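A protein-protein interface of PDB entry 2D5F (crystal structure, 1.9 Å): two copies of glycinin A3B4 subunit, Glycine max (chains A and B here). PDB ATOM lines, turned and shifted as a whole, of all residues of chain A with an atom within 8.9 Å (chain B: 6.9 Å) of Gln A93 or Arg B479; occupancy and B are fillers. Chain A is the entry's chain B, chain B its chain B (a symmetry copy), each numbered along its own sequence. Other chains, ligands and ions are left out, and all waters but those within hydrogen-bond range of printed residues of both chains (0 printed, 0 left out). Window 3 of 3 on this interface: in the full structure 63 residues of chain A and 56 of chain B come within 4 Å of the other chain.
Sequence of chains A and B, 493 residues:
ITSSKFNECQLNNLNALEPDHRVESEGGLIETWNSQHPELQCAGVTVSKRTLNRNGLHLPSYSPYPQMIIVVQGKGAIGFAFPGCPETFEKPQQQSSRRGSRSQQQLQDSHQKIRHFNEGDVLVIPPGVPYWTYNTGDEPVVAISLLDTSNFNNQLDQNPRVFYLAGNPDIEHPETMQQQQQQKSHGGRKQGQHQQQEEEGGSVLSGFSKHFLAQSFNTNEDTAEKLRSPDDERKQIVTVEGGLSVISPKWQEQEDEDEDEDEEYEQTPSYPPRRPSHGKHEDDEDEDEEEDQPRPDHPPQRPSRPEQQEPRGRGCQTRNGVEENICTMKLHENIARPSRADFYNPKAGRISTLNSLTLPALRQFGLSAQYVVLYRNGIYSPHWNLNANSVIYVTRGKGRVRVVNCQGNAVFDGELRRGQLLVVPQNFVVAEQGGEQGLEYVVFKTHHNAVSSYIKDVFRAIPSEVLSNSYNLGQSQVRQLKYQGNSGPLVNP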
ATOM      1  N   GLU A  90      -3.086 -19.094  15.733  1.00  0.00           N
ATOM      2  CA  GLU A  90      -2.254 -20.230  16.109  1.00  0.00           C
ATOM      3  C   GLU A  90      -1.464 -20.774  14.931  1.00  0.00           C
ATOM      4  O   GLU A  90      -1.894 -20.698  13.780  1.00  0.00           O
ATOM      5  CB  GLU A  90      -3.109 -21.334  16.742  1.00  0.00           C
ATOM      6  CG  GLU A  90      -4.194 -21.882  15.847  1.00  0.00           C
ATOM      7  CD  GLU A  90      -5.109 -22.854  16.570  1.00  0.00           C
ATOM      8  OE1 GLU A  90      -6.064 -23.347  15.937  1.00  0.00           O
ATOM      9  OE2 GLU A  90      -4.880 -23.122  17.769  1.00  0.00           O
ATOM     10  N   LYS A  91      -0.293 -21.312  15.234  1.00  0.00           N
ATOM     11  CA  LYS A  91       0.578 -21.864  14.213  1.00  0.00           C
ATOM     12  C   LYS A  91       0.995 -23.275  14.601  1.00  0.00           C
ATOM     13  O   LYS A  91       1.679 -23.472  15.602  1.00  0.00           O
ATOM     14  CB  LYS A  91       1.814 -20.978  14.069  1.00  0.00           C
ATOM     15  CG  LYS A  91       2.790 -21.413  12.996  1.00  0.00           C
ATOM     16  CD  LYS A  91       3.964 -20.452  12.951  1.00  0.00           C
ATOM     17  CE  LYS A  91       4.952 -20.810  11.858  1.00  0.00           C
ATOM     18  NZ  LYS A  91       6.098 -19.848  11.843  1.00  0.00           N
ATOM     19  N   PRO A  92       0.559 -24.280  13.830  1.00  0.00           N
ATOM     20  CA  PRO A  92       0.924 -25.669  14.134  1.00  0.00           C
ATOM     21  C   PRO A  92       2.424 -25.885  13.917  1.00  0.00           C
ATOM     22  O   PRO A  92       3.025 -25.279  13.028  1.00  0.00           O
ATOM     23  CB  PRO A  92       0.080 -26.472  13.147  1.00  0.00           C
ATOM     24  CG  PRO A  92      -1.124 -25.595  12.943  1.00  0.00           C
ATOM     25  CD  PRO A  92      -0.494 -24.232  12.804  1.00  0.00           C
ATOM     26  N   GLN A  93       3.022 -26.747  14.732  1.00  0.00           N
ATOM     27  CA  GLN A  93       4.450 -27.040  14.630  1.00  0.00           C
ATOM     28  C   GLN A  93       4.778 -27.794  13.340  1.00  0.00           C
ATOM     29  O   GLN A  93       3.912 -28.437  12.740  1.00  0.00           O
ATOM     30  CB  GLN A  93       4.889 -27.867  15.841  1.00  0.00           C
ATOM     31  CG  GLN A  93       6.039 -27.276  16.637  1.00  0.00           C
ATOM     32  CD  GLN A  93       6.092 -27.819  18.057  1.00  0.00           C
ATOM     33  OE1 GLN A  93       6.095 -29.037  18.275  1.00  0.00           O
ATOM     34  NE2 GLN A  93       6.131 -26.917  19.035  1.00  0.00           N
ATOM     35  N   GLN A 106       0.114 -30.065  16.830  1.00  0.00           N
ATOM     36  CA  GLN A 106       0.764 -29.544  18.029  1.00  0.00           C
ATOM     37  C   GLN A 106       1.221 -28.105  17.803  1.00  0.00           C
ATOM     38  O   GLN A 106       2.020 -27.828  16.908  1.00  0.00           O
ATOM     39  CB  GLN A 106       1.950 -30.438  18.407  1.00  0.00           C
ATOM     40  CG  GLN A 106       2.302 -31.486  17.354  1.00  0.00           C
ATOM     41  CD  GLN A 106       3.092 -30.912  16.193  1.00  0.00           C
ATOM     42  OE1 GLN A 106       4.269 -30.572  16.339  1.00  0.00           O
ATOM     43  NE2 GLN A 106       2.450 -30.797  15.035  1.00  0.00           N
ATOM     44  N   LEU A 107       0.705 -27.192  18.624  1.00  0.00           N
ATOM     45  CA  LEU A 107       1.023 -25.771  18.504  1.00  0.00           C
ATOM     46  C   LEU A 107       2.477 -25.402  18.744  1.00  0.00           C
ATOM     47  O   LEU A 107       3.085 -25.830  19.723  1.00  0.00           O
ATOM     48  CB  LEU A 107       0.141 -24.942  19.447  1.00  0.00           C
ATOM     49  CG  LEU A 107      -1.307 -24.653  19.031  1.00  0.00           C
ATOM     50  CD1 LEU A 107      -2.075 -25.955  18.837  1.00  0.00           C
ATOM     51  CD2 LEU A 107      -1.974 -23.791  20.099  1.00  0.00           C
ATOM     52  N   GLN A 108       3.017 -24.595  17.833  1.00  0.00           N
ATOM     53  CA  GLN A 108       4.388 -24.109  17.920  1.00  0.00           C
ATOM     54  C   GLN A 108       4.324 -22.763  18.644  1.00  0.00           C
ATOM     55  O   GLN A 108       5.284 -22.325  19.275  1.00  0.00           O
ATOM     56  CB  GLN A 108       4.977 -23.939  16.516  1.00  0.00           C
ATOM     57  CG  GLN A 108       6.379 -23.350  16.482  1.00  0.00           C
ATOM     58  CD  GLN A 108       6.379 -21.831  16.482  1.00  0.00           C
ATOM     59  OE1 GLN A 108       5.904 -21.202  15.533  1.00  0.00           O
ATOM     60  NE2 GLN A 108       6.909 -21.234  17.545  1.00  0.00           N
ATOM     61  N   ASP A 109       3.169 -22.115  18.532  1.00  0.00           N
ATOM     62  CA  ASP A 109       2.910 -20.839  19.184  1.00  0.00           C
ATOM     63  C   ASP A 109       1.478 -20.413  18.904  1.00  0.00           C
ATOM     64  O   ASP A 109       0.883 -20.799  17.894  1.00  0.00           O
ATOM     65  CB  ASP A 109       3.856 -19.738  18.683  1.00  0.00           C
ATOM     66  CG  ASP A 109       3.732 -18.444  19.501  1.00  0.00           C
ATOM     67  OD1 ASP A 109       4.150 -17.371  19.022  1.00  0.00           O
ATOM     68  OD2 ASP A 109       3.224 -18.498  20.637  1.00  0.00           O
ATOM     69  N   SER A 110       0.926 -19.631  19.820  1.00  0.00           N
ATOM     70  CA  SER A 110      -0.416 -19.098  19.674  1.00  0.00           C
ATOM     71  C   SER A 110      -0.449 -17.824  20.502  1.00  0.00           C
ATOM     72  O   SER A 110       0.252 -17.708  21.511  1.00  0.00           O
ATOM     73  CB  SER A 110      -1.475 -20.098  20.162  1.00  0.00           C
ATOM     74  OG  SER A 110      -1.367 -20.348  21.550  1.00  0.00           O
ATOM     75  N   PHE A 217       4.310 -19.195  38.361  1.00  0.00           N
ATOM     76  CA  PHE A 217       4.268 -19.548  36.951  1.00  0.00           C
ATOM     77  C   PHE A 217       4.701 -20.981  36.638  1.00  0.00           C
ATOM     78  O   PHE A 217       4.834 -21.348  35.471  1.00  0.00           O
ATOM     79  CB  PHE A 217       5.135 -18.556  36.164  1.00  0.00           C
ATOM     80  CG  PHE A 217       4.705 -17.117  36.315  1.00  0.00           C
ATOM     81  CD1 PHE A 217       5.640 -16.086  36.232  1.00  0.00           C
ATOM     82  CD2 PHE A 217       3.364 -16.791  36.535  1.00  0.00           C
ATOM     83  CE1 PHE A 217       5.255 -14.757  36.367  1.00  0.00           C
ATOM     84  CE2 PHE A 217       2.964 -15.458  36.672  1.00  0.00           C
ATOM     85  CZ  PHE A 217       3.912 -14.439  36.588  1.00  0.00           C
ATOM     86  N   ASN A 218       4.910 -21.788  37.675  1.00  0.00           N
ATOM     87  CA  ASN A 218       5.324 -23.179  37.492  1.00  0.00           C
ATOM     88  C   ASN A 218       6.506 -23.275  36.536  1.00  0.00           C
ATOM     89  O   ASN A 218       6.475 -24.019  35.558  1.00  0.00           O
ATOM     90  CB  ASN A 218       4.158 -24.016  36.952  1.00  0.00           C
ATOM     91  CG  ASN A 218       4.533 -25.477  36.735  1.00  0.00           C
ATOM     92  OD1 ASN A 218       5.057 -26.140  37.634  1.00  0.00           O
ATOM     93  ND2 ASN A 218       4.258 -25.987  35.538  1.00  0.00           N
ATOM     94  N   THR A 219       7.551 -22.514  36.830  1.00  0.00           N
ATOM     95  CA  THR A 219       8.744 -22.503  36.002  1.00  0.00           C
ATOM     96  C   THR A 219       9.969 -22.633  36.903  1.00  0.00           C
ATOM     97  O   THR A 219       9.837 -22.698  38.124  1.00  0.00           O
ATOM     98  CB  THR A 219       8.831 -21.186  35.208  1.00  0.00           C
ATOM     99  OG1 THR A 219       9.943 -21.238  34.313  1.00  0.00           O
ATOM    100  CG2 THR A 219       9.004 -20.005  36.154  1.00  0.00           C
ATOM    101  N   THR A 223      14.374 -19.056  34.722  1.00  0.00           N
ATOM    102  CA  THR A 223      13.399 -18.369  33.883  1.00  0.00           C
ATOM    103  C   THR A 223      12.766 -17.231  34.682  1.00  0.00           C
ATOM    104  O   THR A 223      12.629 -16.113  34.187  1.00  0.00           O
ATOM    105  CB  THR A 223      12.284 -19.333  33.417  1.00  0.00           C
ATOM    106  OG1 THR A 223      12.857 -20.380  32.626  1.00  0.00           O
ATOM    107  CG2 THR A 223      11.240 -18.594  32.587  1.00  0.00           C
ATOM    108  N   SER B 464       5.173 -15.430  21.070  1.00  0.00           N
ATOM    109  CA  SER B 464       6.386 -16.024  21.601  1.00  0.00           C
ATOM    110  C   SER B 464       7.616 -15.133  21.460  1.00  0.00           C
ATOM    111  O   SER B 464       8.360 -14.947  22.419  1.00  0.00           O
ATOM    112  CB  SER B 464       6.655 -17.364  20.919  1.00  0.00           C
ATOM    113  OG  SER B 464       7.896 -17.885  21.359  1.00  0.00           O
ATOM    114  N   GLY B 474      14.745 -18.024  25.985  1.00  0.00           N
ATOM    115  CA  GLY B 474      14.878 -18.904  24.843  1.00  0.00           C
ATOM    116  C   GLY B 474      13.513 -19.398  24.400  1.00  0.00           C
ATOM    117  O   GLY B 474      12.557 -19.391  25.179  1.00  0.00           O
ATOM    118  N   GLN B 475      13.418 -19.815  23.142  1.00  0.00           N
ATOM    119  CA  GLN B 475      12.174 -20.324  22.589  1.00  0.00           C
ATOM    120  C   GLN B 475      11.565 -21.410  23.477  1.00  0.00           C
ATOM    121  O   GLN B 475      10.356 -21.416  23.713  1.00  0.00           O
ATOM    122  CB  GLN B 475      12.428 -20.854  21.169  1.00  0.00           C
ATOM    123  CG  GLN B 475      11.428 -21.885  20.647  1.00  0.00           C
ATOM    124  CD  GLN B 475       9.988 -21.561  21.006  1.00  0.00           C
ATOM    125  OE1 GLN B 475       9.562 -20.403  20.949  1.00  0.00           O
ATOM    126  NE2 GLN B 475       9.223 -22.591  21.372  1.00  0.00           N
ATOM    127  N   SER B 476      12.396 -22.319  23.979  1.00  0.00           N
ATOM    128  CA  SER B 476      11.899 -23.395  24.834  1.00  0.00           C
ATOM    129  C   SER B 476      11.392 -22.845  26.164  1.00  0.00           C
ATOM    130  O   SER B 476      10.354 -23.275  26.658  1.00  0.00           O
ATOM    131  CB  SER B 476      12.994 -24.443  25.082  1.00  0.00           C
ATOM    132  OG  SER B 476      14.103 -23.886  25.767  1.00  0.00           O
ATOM    133  N   GLN B 477      12.125 -21.897  26.744  1.00  0.00           N
ATOM    134  CA  GLN B 477      11.713 -21.299  28.012  1.00  0.00           C
ATOM    135  C   GLN B 477      10.346 -20.631  27.851  1.00  0.00           C
ATOM    136  O   GLN B 477       9.462 -20.812  28.683  1.00  0.00           O
ATOM    137  CB  GLN B 477      12.742 -20.261  28.483  1.00  0.00           C
ATOM    138  CG  GLN B 477      14.070 -20.842  28.953  1.00  0.00           C
ATOM    139  CD  GLN B 477      15.046 -19.769  29.410  1.00  0.00           C
ATOM    140  OE1 GLN B 477      15.474 -18.927  28.619  1.00  0.00           O
ATOM    141  NE2 GLN B 477      15.401 -19.791  30.694  1.00  0.00           N
ATOM    142  N   VAL B 478      10.182 -19.861  26.779  1.00  0.00           N
ATOM    143  CA  VAL B 478       8.919 -19.176  26.509  1.00  0.00           C
ATOM    144  C   VAL B 478       7.796 -20.191  26.364  1.00  0.00           C
ATOM    145  O   VAL B 478       6.713 -20.032  26.934  1.00  0.00           O
ATOM    146  CB  VAL B 478       9.001 -18.330  25.213  1.00  0.00           C
ATOM    147  CG1 VAL B 478       7.611 -17.828  24.818  1.00  0.00           C
ATOM    148  CG2 VAL B 478       9.936 -17.150  25.425  1.00  0.00           C
ATOM    149  N   ARG B 479       8.067 -21.241  25.598  1.00  0.00           N
ATOM    150  CA  ARG B 479       7.095 -22.297  25.370  1.00  0.00           C
ATOM    151  C   ARG B 479       6.596 -22.907  26.675  1.00  0.00           C
ATOM    152  O   ARG B 479       5.404 -23.167  26.831  1.00  0.00           O
ATOM    153  CB  ARG B 479       7.718 -23.382  24.488  1.00  0.00           C
ATOM    154  CG  ARG B 479       7.059 -24.742  24.592  1.00  0.00           C
ATOM    155  CD  ARG B 479       7.490 -25.612  23.436  1.00  0.00           C
ATOM    156  NE  ARG B 479       6.888 -25.135  22.198  1.00  0.00           N
ATOM    157  CZ  ARG B 479       5.632 -25.380  21.847  1.00  0.00           C
ATOM    158  NH1 ARG B 479       4.850 -26.105  22.639  1.00  0.00           N
ATOM    159  NH2 ARG B 479       5.151 -24.885  20.717  1.00  0.00           N
ATOM    160  N   GLN B 480       7.511 -23.130  27.611  1.00  0.00           N
ATOM    161  CA  GLN B 480       7.151 -23.719  28.894  1.00  0.00           C
ATOM    162  C   GLN B 480       6.285 -22.755  29.711  1.00  0.00           C
ATOM    163  O   GLN B 480       5.423 -23.183  30.476  1.00  0.00           O
ATOM    164  CB  GLN B 480       8.420 -24.100  29.671  1.00  0.00           C
ATOM    165  CG  GLN B 480       8.785 -23.154  30.802  1.00  0.00           C
ATOM    166  CD  GLN B 480       8.497 -23.756  32.161  1.00  0.00           C
ATOM    167  OE1 GLN B 480       7.451 -24.369  32.371  1.00  0.00           O
ATOM    168  NE2 GLN B 480       9.426 -23.583  33.093  1.00  0.00           N
ATOM    169  N   LEU B 481       6.518 -21.455  29.543  1.00  0.00           N
ATOM    170  CA  LEU B 481       5.744 -20.442  30.256  1.00  0.00           C
ATOM    171  C   LEU B 481       4.322 -20.362  29.723  1.00  0.00           C
ATOM    172  O   LEU B 481       3.365 -20.277  30.493  1.00  0.00           O
ATOM    173  CB  LEU B 481       6.386 -19.063  30.113  1.00  0.00           C
ATOM    174  CG  LEU B 481       7.230 -18.500  31.255  1.00  0.00           C
ATOM    175  CD1 LEU B 481       7.507 -17.029  30.963  1.00  0.00           C
ATOM    176  CD2 LEU B 481       6.494 -18.641  32.590  1.00  0.00           C
ATOM    177  N   LYS B 482       4.192 -20.394  28.400  1.00  0.00           N
ATOM    178  CA  LYS B 482       2.892 -20.298  27.751  1.00  0.00           C
ATOM    179  C   LYS B 482       2.059 -21.565  27.741  1.00  0.00           C
ATOM    180  O   LYS B 482       0.828 -21.492  27.731  1.00  0.00           O
ATOM    181  CB  LYS B 482       3.054 -19.825  26.302  1.00  0.00           C
ATOM    182  CG  LYS B 482       3.726 -18.476  26.154  1.00  0.00           C
ATOM    183  CD  LYS B 482       3.729 -18.010  24.707  1.00  0.00           C
ATOM    184  CE  LYS B 482       2.319 -17.736  24.202  1.00  0.00           C
ATOM    185  NZ  LYS B 482       2.340 -17.100  22.858  1.00  0.00           N
ATOM    186  N   TYR B 483       2.700 -22.729  27.759  1.00  0.00           N
ATOM    187  CA  TYR B 483       1.937 -23.969  27.682  1.00  0.00           C
ATOM    188  C   TYR B 483       2.029 -24.982  28.820  1.00  0.00           C
ATOM    189  O   TYR B 483       1.146 -25.824  28.962  1.00  0.00           O
ATOM    190  CB  TYR B 483       2.269 -24.659  26.361  1.00  0.00           C
ATOM    191  CG  TYR B 483       2.114 -23.751  25.161  1.00  0.00           C
ATOM    192  CD1 TYR B 483       0.863 -23.242  24.802  1.00  0.00           C
ATOM    193  CD2 TYR B 483       3.218 -23.392  24.384  1.00  0.00           C
ATOM    194  CE1 TYR B 483       0.715 -22.402  23.703  1.00  0.00           C
ATOM    195  CE2 TYR B 483       3.079 -22.550  23.281  1.00  0.00           C
ATOM    196  CZ  TYR B 483       1.823 -22.061  22.948  1.00  0.00           C
ATOM    197  OH  TYR B 483       1.677 -21.229  21.862  1.00  0.00           O
ATOM    198  N   GLN B 484       3.073 -24.917  29.634  1.00  0.00           N
ATOM    199  CA  GLN B 484       3.200 -25.888  30.717  1.00  0.00           C
ATOM    200  C   GLN B 484       2.592 -25.449  32.044  1.00  0.00           C
ATOM    201  O   GLN B 484       2.588 -24.263  32.385  1.00  0.00           O
ATOM    202  CB  GLN B 484       4.674 -26.268  30.916  1.00  0.00           C
ATOM    203  CG  GLN B 484       5.290 -26.964  29.704  1.00  0.00           C
ATOM    204  CD  GLN B 484       6.693 -27.497  29.963  1.00  0.00           C
ATOM    205  OE1 GLN B 484       7.335 -28.048  29.062  1.00  0.00           O
ATOM    206  NE2 GLN B 484       7.175 -27.338  31.193  1.00  0.00           N
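No position is printed for both chains. Of the 13 pairs that touch across the chains among the printed residues, none has its exchanged pair printed and touching as well.
Of the 12 printed residues of chain B, 8 touch a printed residue of chain A. Printed residues of chain B that touch a printed residue of chain A: Ser B464, Gln B477, Arg B479, Gln B480, Leu B481, Lys B482, Tyr B483 and Gln B484. Hydrophobic or aromatic side chains of chain B that line the printed part of chain A: Leu B481 and Tyr B483. Along chain B the printed residues that touch a printed residue of chain A span positions 464 to 484. Printed residues of chain A that touch a printed residue of chain B: Gln A93, Leu A107, Gln A108, Asp A109, Ser A110, Phe A217, Asn A218, Thr A219 and Thr A223. Hydrophobic or aromatic side chains of chain A that line the printed part of chain B: Phe A217.
NE2 of Gln A93 lies close to NH2 of Arg B479 (2.8 Å). The backbone carbonyl oxygen (O) of Leu A107 sits at hydrogen-bond distance from the guanidinium group (NH2) of Arg B479 (2.5 Å). O of Gln A108 sits at hydrogen-bond distance from NH2 of Arg B479 (2.9 Å). OD1 of Asp A109 is in hydrogen-bond range of N of Ser B464, at 3.0 Å. OD2 of Asp A109 lies within salt-bridge range of NZ of Lys B482, at 2.8 Å. The side-chain carboxylate of Asp A109 sits close to the side-chain hydroxyl of Tyr B483, 3.4 Å away. The backbone carbonyl oxygen (O) of Ser A110 lies within hydrogen-bond range of the side-chain amino group (NZ) of Lys B482 (2.6 Å). The side-chain hydroxyl of Tyr B483 lies within hydrogen-bond range of the backbone NH of Ser A110 (2.7 Å). The backbone carbonyl oxygen (O) of Asn A218 sits close to the side-chain amide oxygen (OE1) of Gln B480 (3.4 Å). The side-chain hydroxyl (OG1) of Thr A219 sits at hydrogen-bond distance from the side-chain amide nitrogen (NE2) of Gln B480, 2.7 Å away. The side-chain hydroxyl (OG1) of Thr A223 lies within hydrogen-bond range of the side-chain amide nitrogen (NE2) of Gln B477, 3.2 Å away.
Among the printed residues, merely in contact across the chains: Phe A217 with Leu B481 (3.8 Å) and Asn A218 with Gln B484 (3.9 Å).
Gln A93 touches one residue of chain B. Printed residues of chain A within 4 Å of Arg B479: Gln A93 (2.8 Å), Leu A107 (2.5 Å) and Gln A108 (2.9 Å). Val B478 touches none of the printed residues of chain A. Of the printed residues of chain A, Ser B464 touches Asp A109. Of the printed residues of chain A, Gln B477 touches Thr A223 (3.2 Å). Of the printed residues of chain A, Leu B481 touches Phe A217. Printed residues of chain A within 4 Å of Gln B480: Asn A218 (3.4 Å) and Thr A219 (2.7 Å). Printed residues of chain B within 4 Å of Gln A108: Arg B479 (2.9 Å). The nearest printed residue of chain A that does not touch Gln B477 is Thr A219 (5.7 Å).
The backbone carbonyl oxygen of Lys A91 is in hydrogen-bond range of the backbone NH of Gln A108, 2.8 Å away. The backbone NH (N) of Lys A91 lies within hydrogen-bond range of the backbone carbonyl oxygen (O) of Asp A109 (3.0 Å). The backbone NH (N) of Gln A93 sits at hydrogen-bond distance from the backbone carbonyl oxygen (O) of Gln A106, 2.6 Å away. The side-chain hydroxyl (OG1) of Thr A223 lies close to the side-chain hydroxyl (OG1) of Thr A219. The side-chain hydroxyl (OG) of Ser B464 lies within hydrogen-bond range of the side-chain amide oxygen (OE1) of Gln B475, 3.0 Å away. N of Gly B474 sits at hydrogen-bond distance from OE1 of Gln B477 (2.9 Å).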
